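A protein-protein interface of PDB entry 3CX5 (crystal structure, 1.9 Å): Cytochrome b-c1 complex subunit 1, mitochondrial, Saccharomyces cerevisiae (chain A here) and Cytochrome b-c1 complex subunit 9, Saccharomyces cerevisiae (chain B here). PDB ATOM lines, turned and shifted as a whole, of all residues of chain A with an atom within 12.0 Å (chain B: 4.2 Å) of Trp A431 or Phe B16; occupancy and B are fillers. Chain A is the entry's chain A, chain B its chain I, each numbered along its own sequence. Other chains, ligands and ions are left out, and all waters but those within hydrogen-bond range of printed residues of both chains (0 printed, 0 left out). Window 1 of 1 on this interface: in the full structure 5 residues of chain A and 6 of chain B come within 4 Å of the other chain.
Thr A329 touches none of the printed residues of chain B.
Gly A397 touches none of the printed residues of chain B.
Printed residues of chain B within 4 Å of Arg A430: Val B17 (3.5 Å).
Of chain B, only Phe B16, Val B17, Gly B18 and Phe B21 come within 4 Å of Trp A431.
Val B15 touches none of the printed residues of chain A.
Of the printed residues of chain A, Phe B16 touches Trp A431 (3.4 Å).
Gly B18 touches one residue of chain A.
No residue of chain A comes within 4 Å of Thr B19.
No residue of chain A comes within 4 Å of Ile B20.
Of the printed residues of chain A, Phe B21 touches Trp A431.
The nearest printed residue of chain B that does not touch Trp A431 is Thr B19 (4.7 Å).
Among the printed residues, merely in contact across the chains: Arg A430 with Val B17 (3.5 Å), Trp A431 with Phe B16 (3.4 Å), Trp A431 with Val B17 (3.4 Å) and Trp A431 with Phe B21 (3.9 Å).
Hydrophobic or aromatic side chains of chain B within 4 Å of the printed part of chain A: Phe B16, Val B17 and Phe B21.
Of the 12 printed residues of chain A, 2 touch a printed residue of chain B.
Hydrophobic or aromatic side chains of chain A that line the printed part of chain B: Trp A431.
The chain-end carboxylate (OXT) of Trp A431 is in hydrogen-bond range of the backbone NH (N) of Gly B18, 3.0 Å away.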
ATOM      1  N   THR A 329      12.758   0.200   3.984  1.00  0.00           N
ATOM      2  CA  THR A 329      12.205   0.808   5.183  1.00  0.00           C
ATOM      3  C   THR A 329      12.475   0.019   6.462  1.00  0.00           C
ATOM      4  O   THR A 329      12.718   0.611   7.514  1.00  0.00           O
ATOM      5  CB  THR A 329      10.683   1.021   5.036  1.00  0.00           C
ATOM      6  OG1 THR A 329      10.445   2.020   4.043  1.00  0.00           O
ATOM      7  CG2 THR A 329      10.040   1.460   6.360  1.00  0.00           C
ATOM      8  N   ILE A 330      12.506  -1.306   6.367  1.00  0.00           N
ATOM      9  CA  ILE A 330      12.671  -2.118   7.567  1.00  0.00           C
ATOM     10  C   ILE A 330      13.892  -3.019   7.750  1.00  0.00           C
ATOM     11  O   ILE A 330      14.302  -3.257   8.881  1.00  0.00           O
ATOM     12  CB  ILE A 330      11.426  -3.023   7.780  1.00  0.00           C
ATOM     13  CG1 ILE A 330      11.259  -3.971   6.590  1.00  0.00           C
ATOM     14  CG2 ILE A 330      10.167  -2.174   7.954  1.00  0.00           C
ATOM     15  CD1 ILE A 330      10.230  -5.057   6.805  1.00  0.00           C
ATOM     16  N   GLY A 397      10.891   5.245   4.402  1.00  0.00           N
ATOM     17  CA  GLY A 397       9.683   5.351   5.201  1.00  0.00           C
ATOM     18  C   GLY A 397       8.866   6.572   4.815  1.00  0.00           C
ATOM     19  O   GLY A 397       7.672   6.655   5.104  1.00  0.00           O
ATOM     20  N   TRP A 401       7.196   3.580   1.698  1.00  0.00           N
ATOM     21  CA  TRP A 401       6.227   2.911   2.552  1.00  0.00           C
ATOM     22  C   TRP A 401       4.811   3.460   2.518  1.00  0.00           C
ATOM     23  O   TRP A 401       4.568   4.614   2.876  1.00  0.00           O
ATOM     24  CB  TRP A 401       6.728   2.851   3.992  1.00  0.00           C
ATOM     25  CG  TRP A 401       5.989   1.837   4.827  1.00  0.00           C
ATOM     26  CD1 TRP A 401       4.856   2.042   5.559  1.00  0.00           C
ATOM     27  CD2 TRP A 401       6.358   0.471   5.034  1.00  0.00           C
ATOM     28  NE1 TRP A 401       4.499   0.891   6.215  1.00  0.00           N
ATOM     29  CE2 TRP A 401       5.406  -0.090   5.913  1.00  0.00           C
ATOM     30  CE3 TRP A 401       7.407  -0.335   4.566  1.00  0.00           C
ATOM     31  CZ2 TRP A 401       5.468  -1.420   6.337  1.00  0.00           C
ATOM     32  CZ3 TRP A 401       7.467  -1.657   4.987  1.00  0.00           C
ATOM     33  CH2 TRP A 401       6.501  -2.184   5.866  1.00  0.00           C
ATOM     34  N   ASP A 402       3.882   2.605   2.090  1.00  0.00           N
ATOM     35  CA  ASP A 402       2.467   2.949   2.000  1.00  0.00           C
ATOM     36  C   ASP A 402       2.234   4.282   1.272  1.00  0.00           C
ATOM     37  O   ASP A 402       1.441   5.116   1.702  1.00  0.00           O
ATOM     38  CB  ASP A 402       1.843   2.943   3.405  1.00  0.00           C
ATOM     39  CG  ASP A 402       0.327   3.009   3.382  1.00  0.00           C
ATOM     40  OD1 ASP A 402      -0.289   2.675   2.348  1.00  0.00           O
ATOM     41  OD2 ASP A 402      -0.257   3.405   4.411  1.00  0.00           O
ATOM     42  N   SER A 424      -1.214  -1.964  -2.723  1.00  0.00           N
ATOM     43  CA  SER A 424      -1.162  -2.627  -1.416  1.00  0.00           C
ATOM     44  C   SER A 424       0.224  -3.196  -1.122  1.00  0.00           C
ATOM     45  O   SER A 424       0.622  -3.325   0.040  1.00  0.00           O
ATOM     46  CB  SER A 424      -2.204  -3.747  -1.325  1.00  0.00           C
ATOM     47  OG  SER A 424      -3.522  -3.216  -1.365  1.00  0.00           O
ATOM     48  N   MET A 426       2.987  -1.820  -1.407  1.00  0.00           N
ATOM     49  CA  MET A 426       3.929  -0.784  -0.989  1.00  0.00           C
ATOM     50  C   MET A 426       4.202  -0.859   0.506  1.00  0.00           C
ATOM     51  O   MET A 426       4.913  -0.020   1.057  1.00  0.00           O
ATOM     52  CB  MET A 426       3.420   0.612  -1.370  1.00  0.00           C
ATOM     53  CG  MET A 426       3.334   0.849  -2.861  1.00  0.00           C
ATOM     54  SD  MET A 426       4.877   0.516  -3.736  1.00  0.00           S
ATOM     55  CE  MET A 426       5.872   1.942  -3.242  1.00  0.00           C
ATOM     56  N   SER A 427       3.629  -1.865   1.160  1.00  0.00           N
ATOM     57  CA  SER A 427       3.821  -2.080   2.592  1.00  0.00           C
ATOM     58  C   SER A 427       3.640  -3.566   2.929  1.00  0.00           C
ATOM     59  O   SER A 427       3.289  -4.365   2.066  1.00  0.00           O
ATOM     60  CB  SER A 427       2.835  -1.237   3.408  1.00  0.00           C
ATOM     61  OG  SER A 427       1.492  -1.630   3.177  1.00  0.00           O
ATOM     62  N   MET A 428       3.903  -3.914   4.184  1.00  0.00           N
ATOM     63  CA  MET A 428       3.769  -5.282   4.687  1.00  0.00           C
ATOM     64  C   MET A 428       2.925  -5.243   5.953  1.00  0.00           C
ATOM     65  O   MET A 428       2.864  -4.214   6.630  1.00  0.00           O
ATOM     66  CB  MET A 428       5.142  -5.849   5.073  1.00  0.00           C
ATOM     67  CG  MET A 428       6.095  -6.117   3.926  1.00  0.00           C
ATOM     68  SD  MET A 428       7.782  -6.350   4.520  1.00  0.00           S
ATOM     69  CE  MET A 428       7.592  -7.786   5.574  1.00  0.00           C
ATOM     70  N   MET A 429       2.293  -6.368   6.279  1.00  0.00           N
ATOM     71  CA  MET A 429       1.498  -6.473   7.496  1.00  0.00           C
ATOM     72  C   MET A 429       2.481  -6.469   8.677  1.00  0.00           C
ATOM     73  O   MET A 429       3.582  -7.011   8.578  1.00  0.00           O
ATOM     74  CB  MET A 429       0.695  -7.780   7.506  1.00  0.00           C
ATOM     75  CG  MET A 429      -0.312  -7.944   6.367  1.00  0.00           C
ATOM     76  SD  MET A 429      -1.652  -6.734   6.388  1.00  0.00           S
ATOM     77  CE  MET A 429      -2.801  -7.523   7.510  1.00  0.00           C
ATOM     78  N   ARG A 430       2.088  -5.833   9.776  1.00  0.00           N
ATOM     79  CA  ARG A 430       2.916  -5.743  10.986  1.00  0.00           C
ATOM     80  C   ARG A 430       2.029  -6.035  12.195  1.00  0.00           C
ATOM     81  O   ARG A 430       0.815  -5.825  12.145  1.00  0.00           O
ATOM     82  CB  ARG A 430       3.465  -4.318  11.167  1.00  0.00           C
ATOM     83  CG  ARG A 430       4.187  -3.696   9.974  1.00  0.00           C
ATOM     84  CD  ARG A 430       5.685  -3.933  10.015  1.00  0.00           C
ATOM     85  NE  ARG A 430       6.049  -5.252   9.508  1.00  0.00           N
ATOM     86  CZ  ARG A 430       7.276  -5.766   9.561  1.00  0.00           C
ATOM     87  NH1 ARG A 430       7.505  -6.975   9.066  1.00  0.00           N
ATOM     88  NH2 ARG A 430       8.269  -5.082  10.121  1.00  0.00           N
ATOM     89  N   TRP A 431       2.632  -6.498  13.287  1.00  0.00           N
ATOM     90  CA  TRP A 431       1.875  -6.759  14.510  1.00  0.00           C
ATOM     91  C   TRP A 431       1.682  -5.439  15.267  1.00  0.00           C
ATOM     92  O   TRP A 431       2.642  -4.635  15.312  1.00  0.00           O
ATOM     93  CB  TRP A 431       2.591  -7.778  15.406  1.00  0.00           C
ATOM     94  CG  TRP A 431       1.869  -8.025  16.711  1.00  0.00           C
ATOM     95  CD1 TRP A 431       2.160  -7.471  17.928  1.00  0.00           C
ATOM     96  CD2 TRP A 431       0.714  -8.855  16.915  1.00  0.00           C
ATOM     97  NE1 TRP A 431       1.256  -7.898  18.873  1.00  0.00           N
ATOM     98  CE2 TRP A 431       0.360  -8.749  18.280  1.00  0.00           C
ATOM     99  CE3 TRP A 431      -0.055  -9.678  16.078  1.00  0.00           C
ATOM    100  CZ2 TRP A 431      -0.732  -9.433  18.827  1.00  0.00           C
ATOM    101  CZ3 TRP A 431      -1.143 -10.359  16.626  1.00  0.00           C
ATOM    102  CH2 TRP A 431      -1.467 -10.230  17.987  1.00  0.00           C
ATOM    103  OXT TRP A 431       0.571  -5.214  15.796  1.00  0.00           O
ATOM    104  N   ALA B  14      -1.965   2.640   8.945  1.00  0.00           N
ATOM    105  CA  ALA B  14      -3.252   2.094   9.344  1.00  0.00           C
ATOM    106  C   ALA B  14      -3.027   1.575  10.763  1.00  0.00           C
ATOM    107  O   ALA B  14      -1.886   1.500  11.221  1.00  0.00           O
ATOM    108  CB  ALA B  14      -3.649   0.948   8.418  1.00  0.00           C
ATOM    109  N   VAL B  15      -4.101   1.252  11.474  1.00  0.00           N
ATOM    110  CA  VAL B  15      -3.964   0.730  12.829  1.00  0.00           C
ATOM    111  C   VAL B  15      -3.506  -0.735  12.756  1.00  0.00           C
ATOM    112  O   VAL B  15      -4.036  -1.522  11.963  1.00  0.00           O
ATOM    113  CB  VAL B  15      -5.295   0.840  13.611  1.00  0.00           C
ATOM    114  CG1 VAL B  15      -5.093   0.430  15.057  1.00  0.00           C
ATOM    115  CG2 VAL B  15      -5.838   2.265  13.531  1.00  0.00           C
ATOM    116  N   PHE B  16      -2.496  -1.081  13.551  1.00  0.00           N
ATOM    117  CA  PHE B  16      -1.960  -2.446  13.576  1.00  0.00           C
ATOM    118  C   PHE B  16      -2.833  -3.408  14.384  1.00  0.00           C
ATOM    119  O   PHE B  16      -3.519  -2.985  15.313  1.00  0.00           O
ATOM    120  CB  PHE B  16      -0.534  -2.444  14.135  1.00  0.00           C
ATOM    121  CG  PHE B  16       0.456  -1.686  13.288  1.00  0.00           C
ATOM    122  CD1 PHE B  16       1.760  -1.494  13.734  1.00  0.00           C
ATOM    123  CD2 PHE B  16       0.094  -1.177  12.043  1.00  0.00           C
ATOM    124  CE1 PHE B  16       2.686  -0.810  12.949  1.00  0.00           C
ATOM    125  CE2 PHE B  16       1.013  -0.493  11.255  1.00  0.00           C
ATOM    126  CZ  PHE B  16       2.309  -0.309  11.707  1.00  0.00           C
ATOM    127  N   VAL B  17      -2.788  -4.696  14.029  1.00  0.00           N
ATOM    128  CA  VAL B  17      -3.572  -5.742  14.705  1.00  0.00           C
ATOM    129  C   VAL B  17      -3.467  -5.723  16.220  1.00  0.00           C
ATOM    130  O   VAL B  17      -4.459  -5.949  16.913  1.00  0.00           O
ATOM    131  CB  VAL B  17      -3.168  -7.170  14.267  1.00  0.00           C
ATOM    132  CG1 VAL B  17      -3.779  -7.515  12.944  1.00  0.00           C
ATOM    133  CG2 VAL B  17      -1.655  -7.296  14.193  1.00  0.00           C
ATOM    134  N   GLY B  18      -2.255  -5.490  16.722  1.00  0.00           N
ATOM    135  CA  GLY B  18      -2.026  -5.458  18.156  1.00  0.00           C
ATOM    136  C   GLY B  18      -2.879  -4.419  18.844  1.00  0.00           C
ATOM    137  O   GLY B  18      -3.478  -4.687  19.883  1.00  0.00           O
ATOM    138  N   THR B  19      -2.960  -3.241  18.237  1.00  0.00           N
ATOM    139  CA  THR B  19      -3.747  -2.136  18.773  1.00  0.00           C
ATOM    140  C   THR B  19      -5.247  -2.363  18.562  1.00  0.00           C
ATOM    141  O   THR B  19      -6.067  -1.937  19.382  1.00  0.00           O
ATOM    142  CB  THR B  19      -3.305  -0.808  18.135  1.00  0.00           C
ATOM    143  OG1 THR B  19      -1.921  -0.591  18.436  1.00  0.00           O
ATOM    144  CG2 THR B  19      -4.132   0.365  18.663  1.00  0.00           C
ATOM    145  N   ILE B  20      -5.597  -3.033  17.462  1.00  0.00           N
ATOM    146  CA  ILE B  20      -6.992  -3.348  17.153  1.00  0.00           C
ATOM    147  C   ILE B  20      -7.532  -4.262  18.251  1.00  0.00           C
ATOM    148  O   ILE B  20      -8.603  -4.014  18.807  1.00  0.00           O
ATOM    149  CB  ILE B  20      -7.125  -4.104  15.792  1.00  0.00           C
ATOM    150  CG1 ILE B  20      -6.730  -3.204  14.620  1.00  0.00           C
ATOM    151  CG2 ILE B  20      -8.551  -4.633  15.611  1.00  0.00           C
ATOM    152  CD1 ILE B  20      -7.650  -2.027  14.411  1.00  0.00           C
ATOM    153  N   PHE B  21      -6.784  -5.325  18.545  1.00  0.00           N
ATOM    154  CA  PHE B  21      -7.168  -6.298  19.567  1.00  0.00           C
ATOM    155  C   PHE B  21      -7.256  -5.660  20.949  1.00  0.00           C
ATOM    156  O   PHE B  21      -8.172  -5.965  21.717  1.00  0.00           O
ATOM    157  CB  PHE B  21      -6.171  -7.462  19.606  1.00  0.00           C
ATOM    158  CG  PHE B  21      -6.284  -8.414  18.443  1.00  0.00           C
ATOM    159  CD1 PHE B  21      -7.379  -8.373  17.584  1.00  0.00           C
ATOM    160  CD2 PHE B  21      -5.297  -9.371  18.222  1.00  0.00           C
ATOM    161  CE1 PHE B  21      -7.492  -9.272  16.522  1.00  0.00           C
ATOM    162  CE2 PHE B  21      -5.402 -10.275  17.164  1.00  0.00           C
ATOM    163  CZ  PHE B  21      -6.501 -10.224  16.312  1.00  0.00           C
